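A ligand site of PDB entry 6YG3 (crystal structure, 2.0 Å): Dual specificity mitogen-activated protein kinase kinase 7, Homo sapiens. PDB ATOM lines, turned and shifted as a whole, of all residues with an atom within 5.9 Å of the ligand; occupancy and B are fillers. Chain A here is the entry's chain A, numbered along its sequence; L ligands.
SG of Cys 104 is covalently linked to C23 of the ligand (1.9 Å). O of Glu 99 sits at hydrogen-bond distance from N5 of the ligand, 2.5 Å away. A nitrogen (N4) of the ligand lies within hydrogen-bond range of the backbone NH of Met 101, at 3.0 Å. A nitrogen (N3) of the ligand is in hydrogen-bond range of the backbone carbonyl oxygen of Met 101. N3 of the ligand lies close to SD of Met 28 (3.7 Å). The backbone carbonyl oxygen (O) of Ser 149 sits at hydrogen-bond distance from a nitrogen (N6) of the ligand (3.1 Å).
N of Lys 107 sits close to SG of Cys 104 (3.6 Å). The backbone NH of Gln 83 is in hydrogen-bond range of the side-chain carboxylate of Glu 99, 2.7 Å away. The backbone carbonyl oxygen (O) of Val 36 is in hydrogen-bond range of the backbone NH (N) of Met 28 (2.8 Å). The backbone carbonyl oxygen (O) of Pro 148 is in hydrogen-bond range of the backbone NH (N) of Glu 106, 3.3 Å away. N of Met 98 is in hydrogen-bond range of O of Ala 49 (2.8 Å). The backbone carbonyl oxygen (O) of Gly 29 lies within hydrogen-bond range of the backbone NH (N) of Val 36 (2.7 Å). N of Cys 162 lies within hydrogen-bond range of O of Asn 150 (3.1 Å). The side-chain hydroxyl (OG) of Ser 30 lies within hydrogen-bond range of the side-chain carboxylate (OE2) of Glu 27.
A nitrogen (N2) of the ligand lies close to the side-chain hydroxyl of Thr 103 (3.3 Å). Glu 27 touches the ligand. Gly 29 touches the ligand. Val 36 touches the ligand. CB of Ala 49 touches N5 of the ligand, at 3.6 Å. CB of Met 98 touches C16 of the ligand, 3.6 Å away. C of Leu 100 touches N4 of the ligand, 3.9 Å away. O of Gly 102 touches C10 of the ligand (3.1 Å). Glu 106 touches the ligand (OE1 to C23, 3.5 Å). CG of Lys 107 touches C5 of the ligand, at 3.6 Å. Leu 152 touches the ligand (CD2 to C20, 3.8 Å). Cys 162 touches the ligand (SG to C19, 3.8 Å). Hydrophobic or aromatic side chains that line the ligand: Met 28, Val 36, Ala 49, Met 98, Met 101 and Leu 152. Within 4 Å of the ligand: Glu 27, Met 28, Gly 29, Val 36, Ala 49, Met 98, Glu 99, Leu 100, Met 101, Gly 102, Thr 103, Cys 104, Glu 106, Lys 107, Ser 149, Leu 152 and Cys 162.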
ATOM      1  N   GLU A  27       0.555  19.873  12.508  1.00  0.00           N
ATOM      2  CA  GLU A  27       0.171  19.706  11.136  1.00  0.00           C
ATOM      3  C   GLU A  27      -1.226  20.232  10.923  1.00  0.00           C
ATOM      4  O   GLU A  27      -2.084  20.002  11.731  1.00  0.00           O
ATOM      5  CB  GLU A  27       0.241  18.222  10.772  1.00  0.00           C
ATOM      6  CG  GLU A  27      -0.237  17.934   9.366  1.00  0.00           C
ATOM      7  CD  GLU A  27      -0.059  16.471   8.965  1.00  0.00           C
ATOM      8  OE1 GLU A  27       1.072  16.011   8.740  1.00  0.00           O
ATOM      9  OE2 GLU A  27      -1.069  15.772   8.852  1.00  0.00           O
ATOM     10  N   MET A  28      -1.449  20.949   9.834  1.00  0.00           N
ATOM     11  CA  MET A  28      -2.763  21.424   9.458  1.00  0.00           C
ATOM     12  C   MET A  28      -3.376  20.646   8.298  1.00  0.00           C
ATOM     13  O   MET A  28      -4.573  20.411   8.290  1.00  0.00           O
ATOM     14  CB  MET A  28      -2.630  22.847   9.050  1.00  0.00           C
ATOM     15  CG  MET A  28      -2.291  23.715  10.212  1.00  0.00           C
ATOM     16  SD  MET A  28      -2.278  25.337   9.536  1.00  0.00           S
ATOM     17  CE  MET A  28      -0.899  25.266   8.395  1.00  0.00           C
ATOM     18  N   GLY A  29      -2.546  20.297   7.301  1.00  0.00           N
ATOM     19  CA  GLY A  29      -2.944  19.347   6.236  1.00  0.00           C
ATOM     20  C   GLY A  29      -1.806  18.387   5.872  1.00  0.00           C
ATOM     21  O   GLY A  29      -0.628  18.666   6.140  1.00  0.00           O
ATOM     22  N   SER A  30      -2.159  17.254   5.274  1.00  0.00           N
ATOM     23  CA  SER A  30      -1.179  16.424   4.571  1.00  0.00           C
ATOM     24  C   SER A  30      -1.938  15.497   3.656  1.00  0.00           C
ATOM     25  O   SER A  30      -3.157  15.402   3.744  1.00  0.00           O
ATOM     26  CB  SER A  30      -0.325  15.591   5.531  1.00  0.00           C
ATOM     27  OG  SER A  30      -1.094  14.609   6.204  1.00  0.00           O
ATOM     28  N   VAL A  36       1.517  20.073   5.443  1.00  0.00           N
ATOM     29  CA  VAL A  36       1.534  21.518   5.784  1.00  0.00           C
ATOM     30  C   VAL A  36       1.519  21.726   7.306  1.00  0.00           C
ATOM     31  O   VAL A  36       0.575  21.314   7.988  1.00  0.00           O
ATOM     32  CB  VAL A  36       0.363  22.268   5.178  1.00  0.00           C
ATOM     33  CG1 VAL A  36       0.470  23.727   5.454  1.00  0.00           C
ATOM     34  CG2 VAL A  36       0.303  22.033   3.670  1.00  0.00           C
ATOM     35  N   ALA A  49       2.389  29.275   7.586  1.00  0.00           N
ATOM     36  CA  ALA A  49       2.203  27.900   7.156  1.00  0.00           C
ATOM     37  C   ALA A  49       3.434  27.526   6.407  1.00  0.00           C
ATOM     38  O   ALA A  49       4.023  28.373   5.680  1.00  0.00           O
ATOM     39  CB  ALA A  49       1.015  27.815   6.208  1.00  0.00           C
ATOM     40  N   VAL A  82      -3.362  32.277  -2.053  1.00  0.00           N
ATOM     41  CA  VAL A  82      -2.444  32.327  -0.902  1.00  0.00           C
ATOM     42  C   VAL A  82      -1.067  32.705  -1.369  1.00  0.00           C
ATOM     43  O   VAL A  82      -0.624  32.283  -2.419  1.00  0.00           O
ATOM     44  CB  VAL A  82      -2.348  30.960  -0.140  1.00  0.00           C
ATOM     45  CG1 VAL A  82      -3.697  30.595   0.444  1.00  0.00           C
ATOM     46  CG2 VAL A  82      -1.881  29.824  -1.037  1.00  0.00           C
ATOM     47  N   GLN A  83      -0.414  33.551  -0.609  1.00  0.00           N
ATOM     48  CA  GLN A  83       0.860  34.045  -1.017  1.00  0.00           C
ATOM     49  C   GLN A  83       2.012  33.275  -0.352  1.00  0.00           C
ATOM     50  O   GLN A  83       1.842  32.660   0.719  1.00  0.00           O
ATOM     51  CB  GLN A  83       0.959  35.551  -0.822  1.00  0.00           C
ATOM     52  CG  GLN A  83       0.236  36.390  -1.973  1.00  0.00           C
ATOM     53  CD  GLN A  83       0.147  35.722  -3.372  1.00  0.00           C
ATOM     54  OE1 GLN A  83       1.127  35.147  -3.894  1.00  0.00           O
ATOM     55  NE2 GLN A  83      -1.042  35.805  -3.996  1.00  0.00           N
ATOM     56  N   MET A  98       4.367  30.174   3.548  1.00  0.00           N
ATOM     57  CA  MET A  98       3.181  30.786   3.055  1.00  0.00           C
ATOM     58  C   MET A  98       2.367  31.404   4.147  1.00  0.00           C
ATOM     59  O   MET A  98       2.494  31.090   5.344  1.00  0.00           O
ATOM     60  CB  MET A  98       2.328  29.755   2.328  1.00  0.00           C
ATOM     61  CG  MET A  98       2.998  29.310   1.030  1.00  0.00           C
ATOM     62  SD  MET A  98       2.106  27.985   0.237  1.00  0.00           S
ATOM     63  CE  MET A  98       2.309  26.690   1.465  1.00  0.00           C
ATOM     64  N   GLU A  99       1.561  32.337   3.716  1.00  0.00           N
ATOM     65  CA  GLU A  99       0.648  33.007   4.590  1.00  0.00           C
ATOM     66  C   GLU A  99      -0.333  31.975   5.144  1.00  0.00           C
ATOM     67  O   GLU A  99      -0.899  31.097   4.422  1.00  0.00           O
ATOM     68  CB  GLU A  99      -0.089  34.166   3.875  1.00  0.00           C
ATOM     69  CG  GLU A  99      -1.414  33.835   3.224  1.00  0.00           C
ATOM     70  CD  GLU A  99      -1.920  35.037   2.442  1.00  0.00           C
ATOM     71  OE1 GLU A  99      -1.904  34.981   1.196  1.00  0.00           O
ATOM     72  OE2 GLU A  99      -2.296  36.043   3.069  1.00  0.00           O
ATOM     73  N   LEU A 100      -0.505  32.081   6.439  1.00  0.00           N
ATOM     74  CA  LEU A 100      -1.381  31.178   7.169  1.00  0.00           C
ATOM     75  C   LEU A 100      -2.847  31.612   7.077  1.00  0.00           C
ATOM     76  O   LEU A 100      -3.160  32.709   7.439  1.00  0.00           O
ATOM     77  CB  LEU A 100      -0.980  31.149   8.633  1.00  0.00           C
ATOM     78  CG  LEU A 100      -1.784  30.239   9.573  1.00  0.00           C
ATOM     79  CD1 LEU A 100      -1.468  28.813   9.271  1.00  0.00           C
ATOM     80  CD2 LEU A 100      -1.416  30.521  11.014  1.00  0.00           C
ATOM     81  N   MET A 101      -3.739  30.702   6.677  1.00  0.00           N
ATOM     82  CA  MET A 101      -5.166  30.968   6.700  1.00  0.00           C
ATOM     83  C   MET A 101      -5.775  30.259   7.903  1.00  0.00           C
ATOM     84  O   MET A 101      -5.105  29.459   8.527  1.00  0.00           O
ATOM     85  CB  MET A 101      -5.811  30.477   5.398  1.00  0.00           C
ATOM     86  CG  MET A 101      -5.313  31.286   4.186  1.00  0.00           C
ATOM     87  SD  MET A 101      -5.704  33.020   4.263  1.00  0.00           S
ATOM     88  CE  MET A 101      -7.409  32.888   3.643  1.00  0.00           C
ATOM     89  N   GLY A 102      -7.015  30.573   8.223  1.00  0.00           N
ATOM     90  CA  GLY A 102      -7.661  30.113   9.489  1.00  0.00           C
ATOM     91  C   GLY A 102      -8.100  28.670   9.412  1.00  0.00           C
ATOM     92  O   GLY A 102      -7.812  27.859  10.288  1.00  0.00           O
ATOM     93  N   THR A 103      -8.823  28.340   8.341  1.00  0.00           N
ATOM     94  CA  THR A 103      -9.204  26.955   8.049  1.00  0.00           C
ATOM     95  C   THR A 103      -9.811  26.890   6.639  1.00  0.00           C
ATOM     96  O   THR A 103      -9.893  27.910   5.952  1.00  0.00           O
ATOM     97  CB  THR A 103     -10.197  26.362   9.085  1.00  0.00           C
ATOM     98  OG1 THR A 103     -10.353  24.942   8.847  1.00  0.00           O
ATOM     99  CG2 THR A 103     -11.497  27.020   8.997  1.00  0.00           C
ATOM    100  N   CYS A 104     -10.216  25.704   6.203  1.00  0.00           N
ATOM    101  CA  CYS A 104     -10.917  25.533   4.930  1.00  0.00           C
ATOM    102  C   CYS A 104     -12.430  25.504   5.058  1.00  0.00           C
ATOM    103  O   CYS A 104     -12.979  25.251   6.175  1.00  0.00           O
ATOM    104  CB  CYS A 104     -10.487  24.222   4.272  1.00  0.00           C
ATOM    105  SG  CYS A 104     -10.821  22.768   5.287  1.00  0.00           S
ATOM    106  N   ALA A 105     -13.113  25.702   3.909  1.00  0.00           N
ATOM    107  CA  ALA A 105     -14.571  25.782   3.893  1.00  0.00           C
ATOM    108  C   ALA A 105     -15.203  24.455   4.327  1.00  0.00           C
ATOM    109  O   ALA A 105     -16.280  24.434   4.939  1.00  0.00           O
ATOM    110  CB  ALA A 105     -15.077  26.200   2.510  1.00  0.00           C
ATOM    111  N   GLU A 106     -14.556  23.346   3.991  1.00  0.00           N
ATOM    112  CA  GLU A 106     -15.005  22.045   4.471  1.00  0.00           C
ATOM    113  C   GLU A 106     -15.081  21.935   6.007  1.00  0.00           C
ATOM    114  O   GLU A 106     -16.084  21.469   6.533  1.00  0.00           O
ATOM    115  CB  GLU A 106     -14.079  20.983   3.948  1.00  0.00           C
ATOM    116  CG  GLU A 106     -14.455  19.577   4.371  1.00  0.00           C
ATOM    117  CD  GLU A 106     -13.330  18.605   4.063  1.00  0.00           C
ATOM    118  OE1 GLU A 106     -12.312  18.604   4.802  1.00  0.00           O
ATOM    119  OE2 GLU A 106     -13.452  17.860   3.055  1.00  0.00           O
ATOM    120  N   LYS A 107     -14.049  22.354   6.725  1.00  0.00           N
ATOM    121  CA  LYS A 107     -14.095  22.422   8.188  1.00  0.00           C
ATOM    122  C   LYS A 107     -15.133  23.362   8.750  1.00  0.00           C
ATOM    123  O   LYS A 107     -15.683  23.107   9.858  1.00  0.00           O
ATOM    124  CB  LYS A 107     -12.758  22.860   8.784  1.00  0.00           C
ATOM    125  CG  LYS A 107     -11.637  21.888   8.549  1.00  0.00           C
ATOM    126  CD  LYS A 107     -12.092  20.437   8.619  1.00  0.00           C
ATOM    127  CE  LYS A 107     -11.010  19.523   8.088  1.00  0.00           C
ATOM    128  NZ  LYS A 107     -11.207  18.157   8.635  1.00  0.00           N
ATOM    129  N   PRO A 148     -14.680  22.546  -1.413  1.00  0.00           N
ATOM    130  CA  PRO A 148     -14.561  23.223  -0.163  1.00  0.00           C
ATOM    131  C   PRO A 148     -13.250  23.030   0.594  1.00  0.00           C
ATOM    132  O   PRO A 148     -12.812  23.939   1.293  1.00  0.00           O
ATOM    133  CB  PRO A 148     -15.736  22.659   0.661  1.00  0.00           C
ATOM    134  CG  PRO A 148     -16.786  22.419  -0.382  1.00  0.00           C
ATOM    135  CD  PRO A 148     -15.999  21.858  -1.534  1.00  0.00           C
ATOM    136  N   SER A 149     -12.620  21.883   0.474  1.00  0.00           N
ATOM    137  CA  SER A 149     -11.354  21.694   1.174  1.00  0.00           C
ATOM    138  C   SER A 149     -10.225  22.590   0.612  1.00  0.00           C
ATOM    139  O   SER A 149      -9.207  22.794   1.286  1.00  0.00           O
ATOM    140  CB  SER A 149     -10.963  20.206   1.166  1.00  0.00           C
ATOM    141  OG  SER A 149     -10.888  19.766  -0.178  1.00  0.00           O
ATOM    142  N   ASN A 150     -10.422  23.121  -0.583  1.00  0.00           N
ATOM    143  CA  ASN A 150      -9.465  23.999  -1.266  1.00  0.00           C
ATOM    144  C   ASN A 150      -9.788  25.482  -1.182  1.00  0.00           C
ATOM    145  O   ASN A 150      -9.166  26.295  -1.843  1.00  0.00           O
ATOM    146  CB  ASN A 150      -9.398  23.604  -2.742  1.00  0.00           C
ATOM    147  CG  ASN A 150      -8.642  22.321  -2.929  1.00  0.00           C
ATOM    148  OD1 ASN A 150      -7.855  21.929  -2.048  1.00  0.00           O
ATOM    149  ND2 ASN A 150      -8.889  21.641  -4.009  1.00  0.00           N
ATOM    150  N   LEU A 152     -10.025  28.597   1.429  1.00  0.00           N
ATOM    151  CA  LEU A 152      -9.488  28.951   2.732  1.00  0.00           C
ATOM    152  C   LEU A 152     -10.060  30.306   3.161  1.00  0.00           C
ATOM    153  O   LEU A 152     -10.301  31.196   2.324  1.00  0.00           O
ATOM    154  CB  LEU A 152      -7.956  28.963   2.730  1.00  0.00           C
ATOM    155  CG  LEU A 152      -7.265  27.662   2.317  1.00  0.00           C
ATOM    156  CD1 LEU A 152      -5.758  27.795   2.208  1.00  0.00           C
ATOM    157  CD2 LEU A 152      -7.614  26.524   3.285  1.00  0.00           C
ATOM    158  N   CYS A 162      -6.627  27.662  -3.040  1.00  0.00           N
ATOM    159  CA  CYS A 162      -5.367  26.978  -2.839  1.00  0.00           C
ATOM    160  C   CYS A 162      -5.281  25.585  -3.554  1.00  0.00           C
ATOM    161  O   CYS A 162      -6.245  25.127  -4.219  1.00  0.00           O
ATOM    162  CB  CYS A 162      -5.128  26.845  -1.323  1.00  0.00           C
ATOM    163  SG  CYS A 162      -5.828  25.362  -0.548  1.00  0.00           S
ATOM    164  N   MET A 300     -15.891  29.399  14.480  1.00  0.00           N
ATOM    165  CA  MET A 300     -14.717  28.694  14.984  1.00  0.00           C
ATOM    166  C   MET A 300     -14.773  28.529  16.520  1.00  0.00           C
ATOM    167  O   MET A 300     -14.085  27.664  17.032  1.00  0.00           O
ATOM    168  CB  MET A 300     -13.411  29.355  14.556  1.00  0.00           C
ATOM    169  CG  MET A 300     -13.154  29.261  13.054  1.00  0.00           C
ATOM    170  SD  MET A 300     -13.200  27.550  12.465  1.00  0.00           S
ATOM    171  CE  MET A 300     -11.521  27.067  12.832  1.00  0.00           C
HETATM  172  C1  LIG L   1      -6.001  19.779  11.599  1.00  0.00           C
HETATM  173  N1  LIG L   1      -6.966  20.840  11.251  1.00  0.00           N
HETATM  174  C2  LIG L   1      -6.509  22.142  11.728  1.00  0.00           C
HETATM  175  C3  LIG L   1      -7.521  23.209  11.405  1.00  0.00           C
HETATM  176  C4  LIG L   1      -7.174  20.888   9.802  1.00  0.00           C
HETATM  177  C5  LIG L   1      -8.166  21.978   9.430  1.00  0.00           C
HETATM  178  N2  LIG L   1      -7.738  23.278   9.952  1.00  0.00           N
HETATM  179  C6  LIG L   1      -6.895  24.139   9.214  1.00  0.00           C
HETATM  180  C7  LIG L   1      -6.684  23.947   7.831  1.00  0.00           C
HETATM  181  C8  LIG L   1      -5.960  24.867   7.094  1.00  0.00           C
HETATM  182  C9  LIG L   1      -6.300  25.238   9.823  1.00  0.00           C
HETATM  183  C10 LIG L   1      -5.583  26.149   9.088  1.00  0.00           C
HETATM  184  C11 LIG L   1      -5.424  25.990   7.714  1.00  0.00           C
HETATM  185  N3  LIG L   1      -4.596  26.952   7.090  1.00  0.00           N
HETATM  186  C12 LIG L   1      -3.902  26.901   5.930  1.00  0.00           C
HETATM  187  N4  LIG L   1      -3.222  27.988   5.574  1.00  0.00           N
HETATM  188  C13 LIG L   1      -2.378  27.878   4.533  1.00  0.00           C
HETATM  189  C14 LIG L   1      -2.193  26.611   3.841  1.00  0.00           C
HETATM  190  C15 LIG L   1      -1.239  26.832   2.788  1.00  0.00           C
HETATM  191  C16 LIG L   1      -0.903  28.144   2.854  1.00  0.00           C
HETATM  192  N5  LIG L   1      -1.569  28.766   3.876  1.00  0.00           N
HETATM  193  C17 LIG L   1      -2.956  25.545   4.347  1.00  0.00           C
HETATM  194  O1  LIG L   1      -2.828  24.283   3.825  1.00  0.00           O
HETATM  195  C18 LIG L   1      -3.973  23.497   3.757  1.00  0.00           C
HETATM  196  C19 LIG L   1      -4.858  23.689   2.704  1.00  0.00           C
HETATM  197  C20 LIG L   1      -6.102  23.091   2.730  1.00  0.00           C
HETATM  198  C21 LIG L   1      -6.492  22.344   3.823  1.00  0.00           C
HETATM  199  N6  LIG L   1      -7.837  21.944   3.879  1.00  0.00           N
HETATM  200  C22 LIG L   1      -8.510  21.335   4.893  1.00  0.00           C
HETATM  201  C23 LIG L   1     -10.005  21.223   4.676  1.00  0.00           C
HETATM  202  O2  LIG L   1      -7.979  21.020   5.951  1.00  0.00           O
HETATM  203  C24 LIG L   1      -5.564  22.092   4.843  1.00  0.00           C
HETATM  204  C25 LIG L   1      -4.305  22.660   4.802  1.00  0.00           C
HETATM  205  N7  LIG L   1      -3.816  25.695   5.349  1.00  0.00           N
